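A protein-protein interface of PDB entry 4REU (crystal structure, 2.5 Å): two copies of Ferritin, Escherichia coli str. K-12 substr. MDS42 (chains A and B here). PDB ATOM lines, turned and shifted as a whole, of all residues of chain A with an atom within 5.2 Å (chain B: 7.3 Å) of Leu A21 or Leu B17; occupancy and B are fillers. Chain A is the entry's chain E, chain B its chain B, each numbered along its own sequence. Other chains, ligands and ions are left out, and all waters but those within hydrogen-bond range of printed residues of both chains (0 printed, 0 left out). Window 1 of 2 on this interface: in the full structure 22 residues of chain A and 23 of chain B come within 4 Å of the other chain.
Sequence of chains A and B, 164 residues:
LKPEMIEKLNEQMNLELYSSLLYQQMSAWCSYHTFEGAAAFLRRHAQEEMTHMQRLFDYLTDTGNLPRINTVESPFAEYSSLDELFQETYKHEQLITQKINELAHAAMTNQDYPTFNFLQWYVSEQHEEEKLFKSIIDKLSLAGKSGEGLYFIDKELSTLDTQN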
ATOM      1  N   LEU A  17      -5.325 -21.167 -13.295  1.00  0.00           N
ATOM      2  CA  LEU A  17      -4.630 -20.431 -14.343  1.00  0.00           C
ATOM      3  C   LEU A  17      -3.961 -19.202 -13.722  1.00  0.00           C
ATOM      4  O   LEU A  17      -2.794 -18.935 -13.926  1.00  0.00           O
ATOM      5  CB  LEU A  17      -5.595 -19.986 -15.446  1.00  0.00           C
ATOM      6  CG  LEU A  17      -5.013 -18.940 -16.414  1.00  0.00           C
ATOM      7  CD1 LEU A  17      -3.751 -19.460 -17.074  1.00  0.00           C
ATOM      8  CD2 LEU A  17      -6.002 -18.577 -17.493  1.00  0.00           C
ATOM      9  N   TYR A  18      -4.711 -18.469 -12.942  1.00  0.00           N
ATOM     10  CA  TYR A  18      -4.175 -17.310 -12.271  1.00  0.00           C
ATOM     11  C   TYR A  18      -2.957 -17.627 -11.400  1.00  0.00           C
ATOM     12  O   TYR A  18      -2.016 -16.846 -11.374  1.00  0.00           O
ATOM     13  CB  TYR A  18      -5.261 -16.638 -11.421  1.00  0.00           C
ATOM     14  CG  TYR A  18      -4.707 -15.571 -10.544  1.00  0.00           C
ATOM     15  CD1 TYR A  18      -4.544 -14.278 -11.026  1.00  0.00           C
ATOM     16  CD2 TYR A  18      -4.289 -15.858  -9.251  1.00  0.00           C
ATOM     17  CE1 TYR A  18      -4.014 -13.274 -10.228  1.00  0.00           C
ATOM     18  CE2 TYR A  18      -3.779 -14.867  -8.437  1.00  0.00           C
ATOM     19  CZ  TYR A  18      -3.639 -13.572  -8.939  1.00  0.00           C
ATOM     20  OH  TYR A  18      -3.110 -12.585  -8.179  1.00  0.00           O
ATOM     21  N   SER A  19      -3.037 -18.728 -10.652  1.00  0.00           N
ATOM     22  CA  SER A  19      -1.961 -19.214  -9.772  1.00  0.00           C
ATOM     23  C   SER A  19      -0.673 -19.489 -10.520  1.00  0.00           C
ATOM     24  O   SER A  19       0.420 -19.097 -10.073  1.00  0.00           O
ATOM     25  CB  SER A  19      -2.397 -20.507  -9.091  1.00  0.00           C
ATOM     26  OG  SER A  19      -3.559 -20.267  -8.337  1.00  0.00           O
ATOM     27  N   SER A  20      -0.821 -20.172 -11.651  1.00  0.00           N
ATOM     28  CA  SER A  20       0.245 -20.334 -12.605  1.00  0.00           C
ATOM     29  C   SER A  20       0.976 -19.024 -12.823  1.00  0.00           C
ATOM     30  O   SER A  20       2.201 -18.958 -12.675  1.00  0.00           O
ATOM     31  CB  SER A  20      -0.284 -20.844 -13.956  1.00  0.00           C
ATOM     32  OG  SER A  20       0.753 -21.467 -14.716  1.00  0.00           O
ATOM     33  N   LEU A  21       0.222 -17.990 -13.179  1.00  0.00           N
ATOM     34  CA  LEU A  21       0.828 -16.729 -13.592  1.00  0.00           C
ATOM     35  C   LEU A  21       1.420 -16.040 -12.371  1.00  0.00           C
ATOM     36  O   LEU A  21       2.472 -15.407 -12.454  1.00  0.00           O
ATOM     37  CB  LEU A  21      -0.178 -15.837 -14.332  1.00  0.00           C
ATOM     38  CG  LEU A  21      -0.810 -16.511 -15.556  1.00  0.00           C
ATOM     39  CD1 LEU A  21      -1.748 -15.549 -16.235  1.00  0.00           C
ATOM     40  CD2 LEU A  21       0.228 -16.972 -16.545  1.00  0.00           C
ATOM     41  N   LEU A  22       0.761 -16.220 -11.234  1.00  0.00           N
ATOM     42  CA  LEU A  22       1.212 -15.631 -10.003  1.00  0.00           C
ATOM     43  C   LEU A  22       2.605 -16.124  -9.716  1.00  0.00           C
ATOM     44  O   LEU A  22       3.494 -15.340  -9.499  1.00  0.00           O
ATOM     45  CB  LEU A  22       0.279 -15.981  -8.868  1.00  0.00           C
ATOM     46  CG  LEU A  22       0.672 -15.396  -7.514  1.00  0.00           C
ATOM     47  CD1 LEU A  22       0.731 -13.879  -7.525  1.00  0.00           C
ATOM     48  CD2 LEU A  22      -0.284 -15.894  -6.452  1.00  0.00           C
ATOM     49  N   TYR A  23       2.808 -17.426  -9.752  1.00  0.00           N
ATOM     50  CA  TYR A  23       4.098 -17.973  -9.384  1.00  0.00           C
ATOM     51  C   TYR A  23       5.179 -17.596 -10.408  1.00  0.00           C
ATOM     52  O   TYR A  23       6.376 -17.490 -10.062  1.00  0.00           O
ATOM     53  CB  TYR A  23       4.000 -19.502  -9.155  1.00  0.00           C
ATOM     54  CG  TYR A  23       3.011 -19.905  -8.062  1.00  0.00           C
ATOM     55  CD1 TYR A  23       2.648 -19.008  -7.042  1.00  0.00           C
ATOM     56  CD2 TYR A  23       2.437 -21.173  -8.040  1.00  0.00           C
ATOM     57  CE1 TYR A  23       1.736 -19.351  -6.062  1.00  0.00           C
ATOM     58  CE2 TYR A  23       1.535 -21.527  -7.057  1.00  0.00           C
ATOM     59  CZ  TYR A  23       1.184 -20.613  -6.069  1.00  0.00           C
ATOM     60  OH  TYR A  23       0.294 -20.938  -5.069  1.00  0.00           O
ATOM     61  N   GLN A  24       4.747 -17.415 -11.659  1.00  0.00           N
ATOM     62  CA  GLN A  24       5.615 -17.007 -12.774  1.00  0.00           C
ATOM     63  C   GLN A  24       6.094 -15.584 -12.521  1.00  0.00           C
ATOM     64  O   GLN A  24       7.273 -15.282 -12.542  1.00  0.00           O
ATOM     65  CB  GLN A  24       4.830 -17.093 -14.076  1.00  0.00           C
ATOM     66  CG  GLN A  24       5.657 -16.880 -15.329  1.00  0.00           C
ATOM     67  CD  GLN A  24       6.434 -18.098 -15.744  1.00  0.00           C
ATOM     68  OE1 GLN A  24       5.884 -19.184 -15.834  1.00  0.00           O
ATOM     69  NE2 GLN A  24       7.727 -17.924 -16.006  1.00  0.00           N
ATOM     70  N   GLN A  25       5.146 -14.719 -12.230  1.00  0.00           N
ATOM     71  CA  GLN A  25       5.425 -13.366 -11.810  1.00  0.00           C
ATOM     72  C   GLN A  25       6.379 -13.313 -10.622  1.00  0.00           C
ATOM     73  O   GLN A  25       7.335 -12.584 -10.649  1.00  0.00           O
ATOM     74  CB  GLN A  25       4.124 -12.667 -11.426  1.00  0.00           C
ATOM     75  CG  GLN A  25       4.314 -11.202 -11.064  1.00  0.00           C
ATOM     76  CD  GLN A  25       4.936 -10.410 -12.205  1.00  0.00           C
ATOM     77  OE1 GLN A  25       6.093  -9.986 -12.157  1.00  0.00           O
ATOM     78  NE2 GLN A  25       4.198 -10.289 -13.266  1.00  0.00           N
ATOM     79  N   MET A  26       6.076 -14.073  -9.574  1.00  0.00           N
ATOM     80  CA  MET A  26       6.895 -14.151  -8.382  1.00  0.00           C
ATOM     81  C   MET A  26       8.298 -14.638  -8.721  1.00  0.00           C
ATOM     82  O   MET A  26       9.269 -14.212  -8.128  1.00  0.00           O
ATOM     83  CB  MET A  26       6.265 -15.134  -7.394  1.00  0.00           C
ATOM     84  CG  MET A  26       5.074 -14.598  -6.619  1.00  0.00           C
ATOM     85  SD  MET A  26       4.388 -15.913  -5.587  1.00  0.00           S
ATOM     86  CE  MET A  26       3.303 -14.959  -4.512  1.00  0.00           C
ATOM     87  N   VAL A  72      -7.772 -12.503 -16.660  1.00  0.00           N
ATOM     88  CA  VAL A  72      -6.852 -12.677 -15.564  1.00  0.00           C
ATOM     89  C   VAL A  72      -6.375 -11.343 -14.951  1.00  0.00           C
ATOM     90  O   VAL A  72      -5.769 -10.552 -15.649  1.00  0.00           O
ATOM     91  CB  VAL A  72      -5.574 -13.356 -16.053  1.00  0.00           C
ATOM     92  CG1 VAL A  72      -4.707 -13.735 -14.848  1.00  0.00           C
ATOM     93  CG2 VAL A  72      -5.896 -14.567 -16.908  1.00  0.00           C
ATOM     94  N   PRO A  75      -0.934 -10.373 -11.739  1.00  0.00           N
ATOM     95  CA  PRO A  75      -0.313 -10.832 -10.504  1.00  0.00           C
ATOM     96  C   PRO A  75       0.819  -9.934 -10.040  1.00  0.00           C
ATOM     97  O   PRO A  75       1.517 -10.280  -9.090  1.00  0.00           O
ATOM     98  CB  PRO A  75       0.259 -12.211 -10.886  1.00  0.00           C
ATOM     99  CG  PRO A  75       0.601 -12.087 -12.324  1.00  0.00           C
ATOM    100  CD  PRO A  75      -0.405 -11.099 -12.912  1.00  0.00           C
ATOM    101  N   GLU B  11       5.733  -6.221 -23.446  1.00  0.00           N
ATOM    102  CA  GLU B  11       4.417  -6.274 -24.062  1.00  0.00           C
ATOM    103  C   GLU B  11       4.282  -7.495 -25.003  1.00  0.00           C
ATOM    104  O   GLU B  11       3.228  -8.094 -25.084  1.00  0.00           O
ATOM    105  CB  GLU B  11       4.127  -4.956 -24.800  1.00  0.00           C
ATOM    106  CG  GLU B  11       2.667  -4.765 -25.251  1.00  0.00           C
ATOM    107  CD  GLU B  11       1.569  -5.005 -24.163  1.00  0.00           C
ATOM    108  OE1 GLU B  11       1.803  -4.781 -22.935  1.00  0.00           O
ATOM    109  OE2 GLU B  11       0.431  -5.415 -24.547  1.00  0.00           O
ATOM    110  N   GLN B  12       5.334  -7.831 -25.728  1.00  0.00           N
ATOM    111  CA  GLN B  12       5.335  -8.988 -26.576  1.00  0.00           C
ATOM    112  C   GLN B  12       5.257 -10.242 -25.709  1.00  0.00           C
ATOM    113  O   GLN B  12       4.626 -11.215 -26.065  1.00  0.00           O
ATOM    114  CB  GLN B  12       6.631  -9.033 -27.364  1.00  0.00           C
ATOM    115  CG  GLN B  12       6.697 -10.130 -28.408  1.00  0.00           C
ATOM    116  CD  GLN B  12       5.665  -9.958 -29.522  1.00  0.00           C
ATOM    117  OE1 GLN B  12       5.239  -8.848 -29.841  1.00  0.00           O
ATOM    118  NE2 GLN B  12       5.269 -11.069 -30.121  1.00  0.00           N
ATOM    119  N   MET B  13       5.916 -10.211 -24.559  1.00  0.00           N
ATOM    120  CA  MET B  13       5.799 -11.311 -23.628  1.00  0.00           C
ATOM    121  C   MET B  13       4.320 -11.549 -23.296  1.00  0.00           C
ATOM    122  O   MET B  13       3.836 -12.707 -23.248  1.00  0.00           O
ATOM    123  CB  MET B  13       6.589 -11.027 -22.348  1.00  0.00           C
ATOM    124  CG  MET B  13       6.412 -12.124 -21.288  1.00  0.00           C
ATOM    125  SD  MET B  13       7.149 -11.746 -19.692  1.00  0.00           S
ATOM    126  CE  MET B  13       5.923 -10.551 -19.162  1.00  0.00           C
ATOM    127  N   ASN B  14       3.633 -10.452 -23.027  1.00  0.00           N
ATOM    128  CA  ASN B  14       2.213 -10.498 -22.711  1.00  0.00           C
ATOM    129  C   ASN B  14       1.343 -10.982 -23.869  1.00  0.00           C
ATOM    130  O   ASN B  14       0.438 -11.760 -23.649  1.00  0.00           O
ATOM    131  CB  ASN B  14       1.730  -9.158 -22.194  1.00  0.00           C
ATOM    132  CG  ASN B  14       2.002  -9.010 -20.718  1.00  0.00           C
ATOM    133  OD1 ASN B  14       1.259  -9.516 -19.895  1.00  0.00           O
ATOM    134  ND2 ASN B  14       3.101  -8.356 -20.376  1.00  0.00           N
ATOM    135  N   LEU B  15       1.662 -10.547 -25.085  1.00  0.00           N
ATOM    136  CA  LEU B  15       1.013 -11.021 -26.282  1.00  0.00           C
ATOM    137  C   LEU B  15       1.296 -12.522 -26.484  1.00  0.00           C
ATOM    138  O   LEU B  15       0.446 -13.285 -26.917  1.00  0.00           O
ATOM    139  CB  LEU B  15       1.542 -10.228 -27.449  1.00  0.00           C
ATOM    140  CG  LEU B  15       0.963 -10.554 -28.816  1.00  0.00           C
ATOM    141  CD1 LEU B  15      -0.556 -10.391 -28.856  1.00  0.00           C
ATOM    142  CD2 LEU B  15       1.615  -9.656 -29.861  1.00  0.00           C
ATOM    143  N   GLU B  16       2.504 -12.962 -26.183  1.00  0.00           N
ATOM    144  CA  GLU B  16       2.801 -14.366 -26.342  1.00  0.00           C
ATOM    145  C   GLU B  16       1.960 -15.220 -25.369  1.00  0.00           C
ATOM    146  O   GLU B  16       1.540 -16.325 -25.723  1.00  0.00           O
ATOM    147  CB  GLU B  16       4.302 -14.633 -26.209  1.00  0.00           C
ATOM    148  CG  GLU B  16       5.087 -13.977 -27.323  1.00  0.00           C
ATOM    149  CD  GLU B  16       5.008 -14.691 -28.659  1.00  0.00           C
ATOM    150  OE1 GLU B  16       5.491 -14.077 -29.636  1.00  0.00           O
ATOM    151  OE2 GLU B  16       4.515 -15.846 -28.743  1.00  0.00           O
ATOM    152  N   LEU B  17       1.703 -14.665 -24.179  1.00  0.00           N
ATOM    153  CA  LEU B  17       0.870 -15.287 -23.116  1.00  0.00           C
ATOM    154  C   LEU B  17      -0.604 -15.360 -23.506  1.00  0.00           C
ATOM    155  O   LEU B  17      -1.260 -16.430 -23.393  1.00  0.00           O
ATOM    156  CB  LEU B  17       0.998 -14.492 -21.811  1.00  0.00           C
ATOM    157  CG  LEU B  17       0.150 -14.902 -20.616  1.00  0.00           C
ATOM    158  CD1 LEU B  17       0.295 -16.380 -20.310  1.00  0.00           C
ATOM    159  CD2 LEU B  17       0.557 -14.134 -19.377  1.00  0.00           C
ATOM    160  N   TYR B  18      -1.118 -14.227 -23.980  1.00  0.00           N
ATOM    161  CA  TYR B  18      -2.468 -14.171 -24.520  1.00  0.00           C
ATOM    162  C   TYR B  18      -2.664 -15.244 -25.626  1.00  0.00           C
ATOM    163  O   TYR B  18      -3.714 -15.882 -25.705  1.00  0.00           O
ATOM    164  CB  TYR B  18      -2.788 -12.749 -25.026  1.00  0.00           C
ATOM    165  CG  TYR B  18      -4.152 -12.664 -25.675  1.00  0.00           C
ATOM    166  CD1 TYR B  18      -4.326 -12.967 -27.031  1.00  0.00           C
ATOM    167  CD2 TYR B  18      -5.259 -12.382 -24.939  1.00  0.00           C
ATOM    168  CE1 TYR B  18      -5.565 -12.930 -27.624  1.00  0.00           C
ATOM    169  CE2 TYR B  18      -6.498 -12.318 -25.522  1.00  0.00           C
ATOM    170  CZ  TYR B  18      -6.652 -12.607 -26.869  1.00  0.00           C
ATOM    171  OH  TYR B  18      -7.911 -12.579 -27.443  1.00  0.00           O
ATOM    172  N   SER B  19      -1.650 -15.435 -26.464  1.00  0.00           N
ATOM    173  CA  SER B  19      -1.754 -16.339 -27.579  1.00  0.00           C
ATOM    174  C   SER B  19      -1.850 -17.752 -27.053  1.00  0.00           C
ATOM    175  O   SER B  19      -2.637 -18.561 -27.581  1.00  0.00           O
ATOM    176  CB  SER B  19      -0.549 -16.188 -28.537  1.00  0.00           C
ATOM    177  OG  SER B  19      -0.446 -14.849 -28.988  1.00  0.00           O
ATOM    178  N   SER B  20      -1.056 -18.055 -26.027  1.00  0.00           N
ATOM    179  CA  SER B  20      -1.212 -19.352 -25.312  1.00  0.00           C
ATOM    180  C   SER B  20      -2.663 -19.616 -24.886  1.00  0.00           C
ATOM    181  O   SER B  20      -3.203 -20.677 -25.142  1.00  0.00           O
ATOM    182  CB  SER B  20      -0.314 -19.470 -24.082  1.00  0.00           C
ATOM    183  OG  SER B  20      -0.207 -20.828 -23.616  1.00  0.00           O
ATOM    184  N   LEU B  21      -3.278 -18.643 -24.249  1.00  0.00           N
ATOM    185  CA  LEU B  21      -4.617 -18.796 -23.723  1.00  0.00           C
ATOM    186  C   LEU B  21      -5.685 -18.823 -24.826  1.00  0.00           C
ATOM    187  O   LEU B  21      -6.746 -19.465 -24.701  1.00  0.00           O
ATOM    188  CB  LEU B  21      -4.899 -17.689 -22.686  1.00  0.00           C
ATOM    189  CG  LEU B  21      -3.938 -17.649 -21.510  1.00  0.00           C
ATOM    190  CD1 LEU B  21      -4.369 -16.578 -20.527  1.00  0.00           C
ATOM    191  CD2 LEU B  21      -3.877 -18.978 -20.770  1.00  0.00           C
ATOM    192  N   LEU B  22      -5.400 -18.117 -25.899  1.00  0.00           N
ATOM    193  CA  LEU B  22      -6.317 -18.046 -27.024  1.00  0.00           C
ATOM    194  C   LEU B  22      -6.417 -19.408 -27.701  1.00  0.00           C
ATOM    195  O   LEU B  22      -7.502 -19.836 -28.065  1.00  0.00           O
ATOM    196  CB  LEU B  22      -5.817 -17.009 -28.010  1.00  0.00           C
ATOM    197  CG  LEU B  22      -6.571 -16.964 -29.324  1.00  0.00           C
ATOM    198  CD1 LEU B  22      -8.020 -16.492 -29.146  1.00  0.00           C
ATOM    199  CD2 LEU B  22      -5.780 -16.085 -30.291  1.00  0.00           C
ATOM    200  N   TYR B  23      -5.281 -20.072 -27.869  1.00  0.00           N
ATOM    201  CA  TYR B  23      -5.258 -21.350 -28.526  1.00  0.00           C
ATOM    202  C   TYR B  23      -5.854 -22.399 -27.598  1.00  0.00           C
ATOM    203  O   TYR B  23      -6.606 -23.236 -28.046  1.00  0.00           O
ATOM    204  CB  TYR B  23      -3.837 -21.716 -29.039  1.00  0.00           C
ATOM    205  CG  TYR B  23      -3.257 -20.718 -30.049  1.00  0.00           C
ATOM    206  CD1 TYR B  23      -4.069 -19.856 -30.763  1.00  0.00           C
ATOM    207  CD2 TYR B  23      -1.891 -20.650 -30.292  1.00  0.00           C
ATOM    208  CE1 TYR B  23      -3.551 -18.958 -31.669  1.00  0.00           C
ATOM    209  CE2 TYR B  23      -1.359 -19.744 -31.211  1.00  0.00           C
ATOM    210  CZ  TYR B  23      -2.204 -18.895 -31.873  1.00  0.00           C
ATOM    211  OH  TYR B  23      -1.712 -17.993 -32.757  1.00  0.00           O
ATOM    212  N   ALA B  46      -0.649 -24.180 -27.770  1.00  0.00           N
ATOM    213  CA  ALA B  46      -0.738 -23.316 -26.621  1.00  0.00           C
ATOM    214  C   ALA B  46       0.510 -23.448 -25.781  1.00  0.00           C
ATOM    215  O   ALA B  46       0.980 -22.483 -25.227  1.00  0.00           O
ATOM    216  CB  ALA B  46      -1.958 -23.685 -25.794  1.00  0.00           C
ATOM    217  N   GLU B  49       3.408 -21.580 -27.432  1.00  0.00           N
ATOM    218  CA  GLU B  49       3.285 -20.177 -27.147  1.00  0.00           C
ATOM    219  C   GLU B  49       3.776 -19.842 -25.754  1.00  0.00           C
ATOM    220  O   GLU B  49       4.492 -18.868 -25.610  1.00  0.00           O
ATOM    221  CB  GLU B  49       1.878 -19.708 -27.401  1.00  0.00           C
ATOM    222  CG  GLU B  49       1.445 -19.886 -28.866  1.00  0.00           C
ATOM    223  CD  GLU B  49       2.169 -18.952 -29.839  1.00  0.00           C
ATOM    224  OE1 GLU B  49       2.878 -17.993 -29.411  1.00  0.00           O
ATOM    225  OE2 GLU B  49       2.008 -19.167 -31.048  1.00  0.00           O
ATOM    226  N   MET B  50       3.514 -20.674 -24.748  1.00  0.00           N
ATOM    227  CA  MET B  50       4.085 -20.415 -23.388  1.00  0.00           C
ATOM    228  C   MET B  50       5.582 -20.402 -23.370  1.00  0.00           C
ATOM    229  O   MET B  50       6.194 -19.697 -22.585  1.00  0.00           O
ATOM    230  CB  MET B  50       3.673 -21.456 -22.354  1.00  0.00           C
ATOM    231  CG  MET B  50       2.377 -21.105 -21.685  1.00  0.00           C
ATOM    232  SD  MET B  50       2.397 -19.552 -20.758  1.00  0.00           S
ATOM    233  CE  MET B  50       0.659 -19.648 -20.377  1.00  0.00           C
ATOM    234  N   HIS B  52       7.446 -19.413 -25.898  1.00  0.00           N
ATOM    235  CA  HIS B  52       7.814 -18.149 -26.515  1.00  0.00           C
ATOM    236  C   HIS B  52       7.724 -17.082 -25.466  1.00  0.00           C
ATOM    237  O   HIS B  52       8.557 -16.203 -25.385  1.00  0.00           O
ATOM    238  CB  HIS B  52       6.845 -17.765 -27.628  1.00  0.00           C
ATOM    239  CG  HIS B  52       6.830 -18.710 -28.773  1.00  0.00           C
ATOM    240  ND1 HIS B  52       5.975 -18.560 -29.843  1.00  0.00           N
ATOM    241  CD2 HIS B  52       7.560 -19.815 -29.027  1.00  0.00           C
ATOM    242  CE1 HIS B  52       6.178 -19.532 -30.710  1.00  0.00           C
ATOM    243  NE2 HIS B  52       7.140 -20.304 -30.239  1.00  0.00           N
ATOM    244  N   MET B  53       6.671 -17.165 -24.677  1.00  0.00           N
ATOM    245  CA  MET B  53       6.472 -16.256 -23.571  1.00  0.00           C
ATOM    246  C   MET B  53       7.680 -16.264 -22.649  1.00  0.00           C
ATOM    247  O   MET B  53       8.178 -15.192 -22.287  1.00  0.00           O
ATOM    248  CB  MET B  53       5.212 -16.622 -22.811  1.00  0.00           C
ATOM    249  CG  MET B  53       4.872 -15.654 -21.707  1.00  0.00           C
ATOM    250  SD  MET B  53       5.541 -16.048 -20.066  1.00  0.00           S
ATOM    251  CE  MET B  53       3.935 -16.268 -19.309  1.00  0.00           C
ATOM    252  N   GLN B  54       8.146 -17.466 -22.297  1.00  0.00           N
ATOM    253  CA  GLN B  54       9.211 -17.647 -21.308  1.00  0.00           C
ATOM    254  C   GLN B  54      10.562 -17.213 -21.855  1.00  0.00           C
ATOM    255  O   GLN B  54      11.401 -16.688 -21.116  1.00  0.00           O
ATOM    256  CB  GLN B  54       9.239 -19.103 -20.778  1.00  0.00           C
ATOM    257  CG  GLN B  54       8.050 -19.403 -19.852  1.00  0.00           C
ATOM    258  CD  GLN B  54       7.748 -20.897 -19.602  1.00  0.00           C
ATOM    259  OE1 GLN B  54       7.768 -21.730 -20.530  1.00  0.00           O
ATOM    260  NE2 GLN B  54       7.419 -21.231 -18.340  1.00  0.00           N
ATOM    261  N   PHE B  57      10.426 -13.577 -21.226  1.00  0.00           N
ATOM    262  CA  PHE B  57      10.560 -13.480 -19.790  1.00  0.00           C
ATOM    263  C   PHE B  57      12.034 -13.537 -19.405  1.00  0.00           C
ATOM    264  O   PHE B  57      12.521 -12.678 -18.723  1.00  0.00           O
ATOM    265  CB  PHE B  57       9.809 -14.629 -19.169  1.00  0.00           C
ATOM    266  CG  PHE B  57       9.676 -14.561 -17.680  1.00  0.00           C
ATOM    267  CD1 PHE B  57      10.742 -14.918 -16.852  1.00  0.00           C
ATOM    268  CD2 PHE B  57       8.475 -14.201 -17.095  1.00  0.00           C
ATOM    269  CE1 PHE B  57      10.615 -14.901 -15.476  1.00  0.00           C
ATOM    270  CE2 PHE B  57       8.340 -14.175 -15.714  1.00  0.00           C
ATOM    271  CZ  PHE B  57       9.407 -14.537 -14.910  1.00  0.00           C
ATOM    272  N   ILE B  69       3.589  -9.109 -15.913  1.00  0.00           N
ATOM    273  CA  ILE B  69       2.412  -9.717 -16.451  1.00  0.00           C
ATOM    274  C   ILE B  69       1.239  -8.784 -16.165  1.00  0.00           C
ATOM    275  O   ILE B  69       0.880  -8.572 -15.017  1.00  0.00           O
ATOM    276  CB  ILE B  69       2.167 -11.084 -15.773  1.00  0.00           C
ATOM    277  CG1 ILE B  69       3.329 -12.012 -16.096  1.00  0.00           C
ATOM    278  CG2 ILE B  69       0.863 -11.721 -16.227  1.00  0.00           C
ATOM    279  CD1 ILE B  69       3.164 -13.422 -15.568  1.00  0.00           C
ATOM    280  N   ASN B  70       0.623  -8.315 -17.243  1.00  0.00           N
ATOM    281  CA  ASN B  70      -0.440  -7.366 -17.201  1.00  0.00           C
ATOM    282  C   ASN B  70      -1.808  -8.065 -17.189  1.00  0.00           C
ATOM    283  O   ASN B  70      -1.914  -9.298 -17.253  1.00  0.00           O
ATOM    284  CB  ASN B  70      -0.304  -6.427 -18.410  1.00  0.00           C
ATOM    285  CG  ASN B  70       1.016  -5.638 -18.401  1.00  0.00           C
ATOM    286  OD1 ASN B  70       1.449  -5.117 -17.358  1.00  0.00           O
ATOM    287  ND2 ASN B  70       1.658  -5.549 -19.554  1.00  0.00           N
ATOM    288  N   VAL B  72      -4.773  -9.820 -18.413  1.00  0.00           N
ATOM    289  CA  VAL B  72      -4.945 -10.603 -19.634  1.00  0.00           C
ATOM    290  C   VAL B  72      -6.419 -10.652 -20.009  1.00  0.00           C
ATOM    291  O   VAL B  72      -7.231 -11.218 -19.298  1.00  0.00           O
ATOM    292  CB  VAL B  72      -4.397 -12.028 -19.496  1.00  0.00           C
ATOM    293  CG1 VAL B  72      -4.274 -12.687 -20.854  1.00  0.00           C
ATOM    294  CG2 VAL B  72      -3.033 -12.014 -18.843  1.00  0.00           C
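Leu A17 touches Leu B21, and with the chains exchanged Leu A21 touches Leu B17.
Val A72 touches its own counterpart, Val B72.
8 positions are printed for both chains.
Of the 23 printed residues of chain B, 6 touch a printed residue of chain A.
Hydrophobic or aromatic side chains of chain A within 4 Å of the printed part of chain B: Leu A17, Leu A21, Val A72 and Pro A75.
Among the printed residues, 8 pairs touch across the chains.
Among the printed residues, no Asp or Glu carboxylate lies within 4 Å of a Lys or Arg side-chain nitrogen of the other chain.
Leu A21 touches just these residues of chain B: Leu B17 (3.8 Å) and Ile B69 (3.8 Å).
Leu B17 touches one residue of chain A.
Printed residues of chain A within 4 Å of Phe B57: Gln A24.
Of the printed residues of chain A, Val B72 touches Val A72.
The backbone carbonyl oxygen of Met B50 sits close to the side-chain amide oxygen of Gln B54 (3.3 Å).
Among the printed residues, merely in contact across the chains: Leu A17 with Leu B21 (3.7 Å), Leu A21 with Leu B17 (3.8 Å), Leu A21 with Ile B69 (3.8 Å), Gln A24 with Gln B54 (3.6 Å), Gln A24 with Phe B57 (3.3 Å) and Pro A75 with Ile B69 (3.5 Å).
NE2 of Gln A25 sits close to N of Ile B69, at 3.0 Å.
The backbone carbonyl oxygen (O) of Val B72 is in hydrogen-bond range of the backbone NH (N) of Val A72 (3.0 Å).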
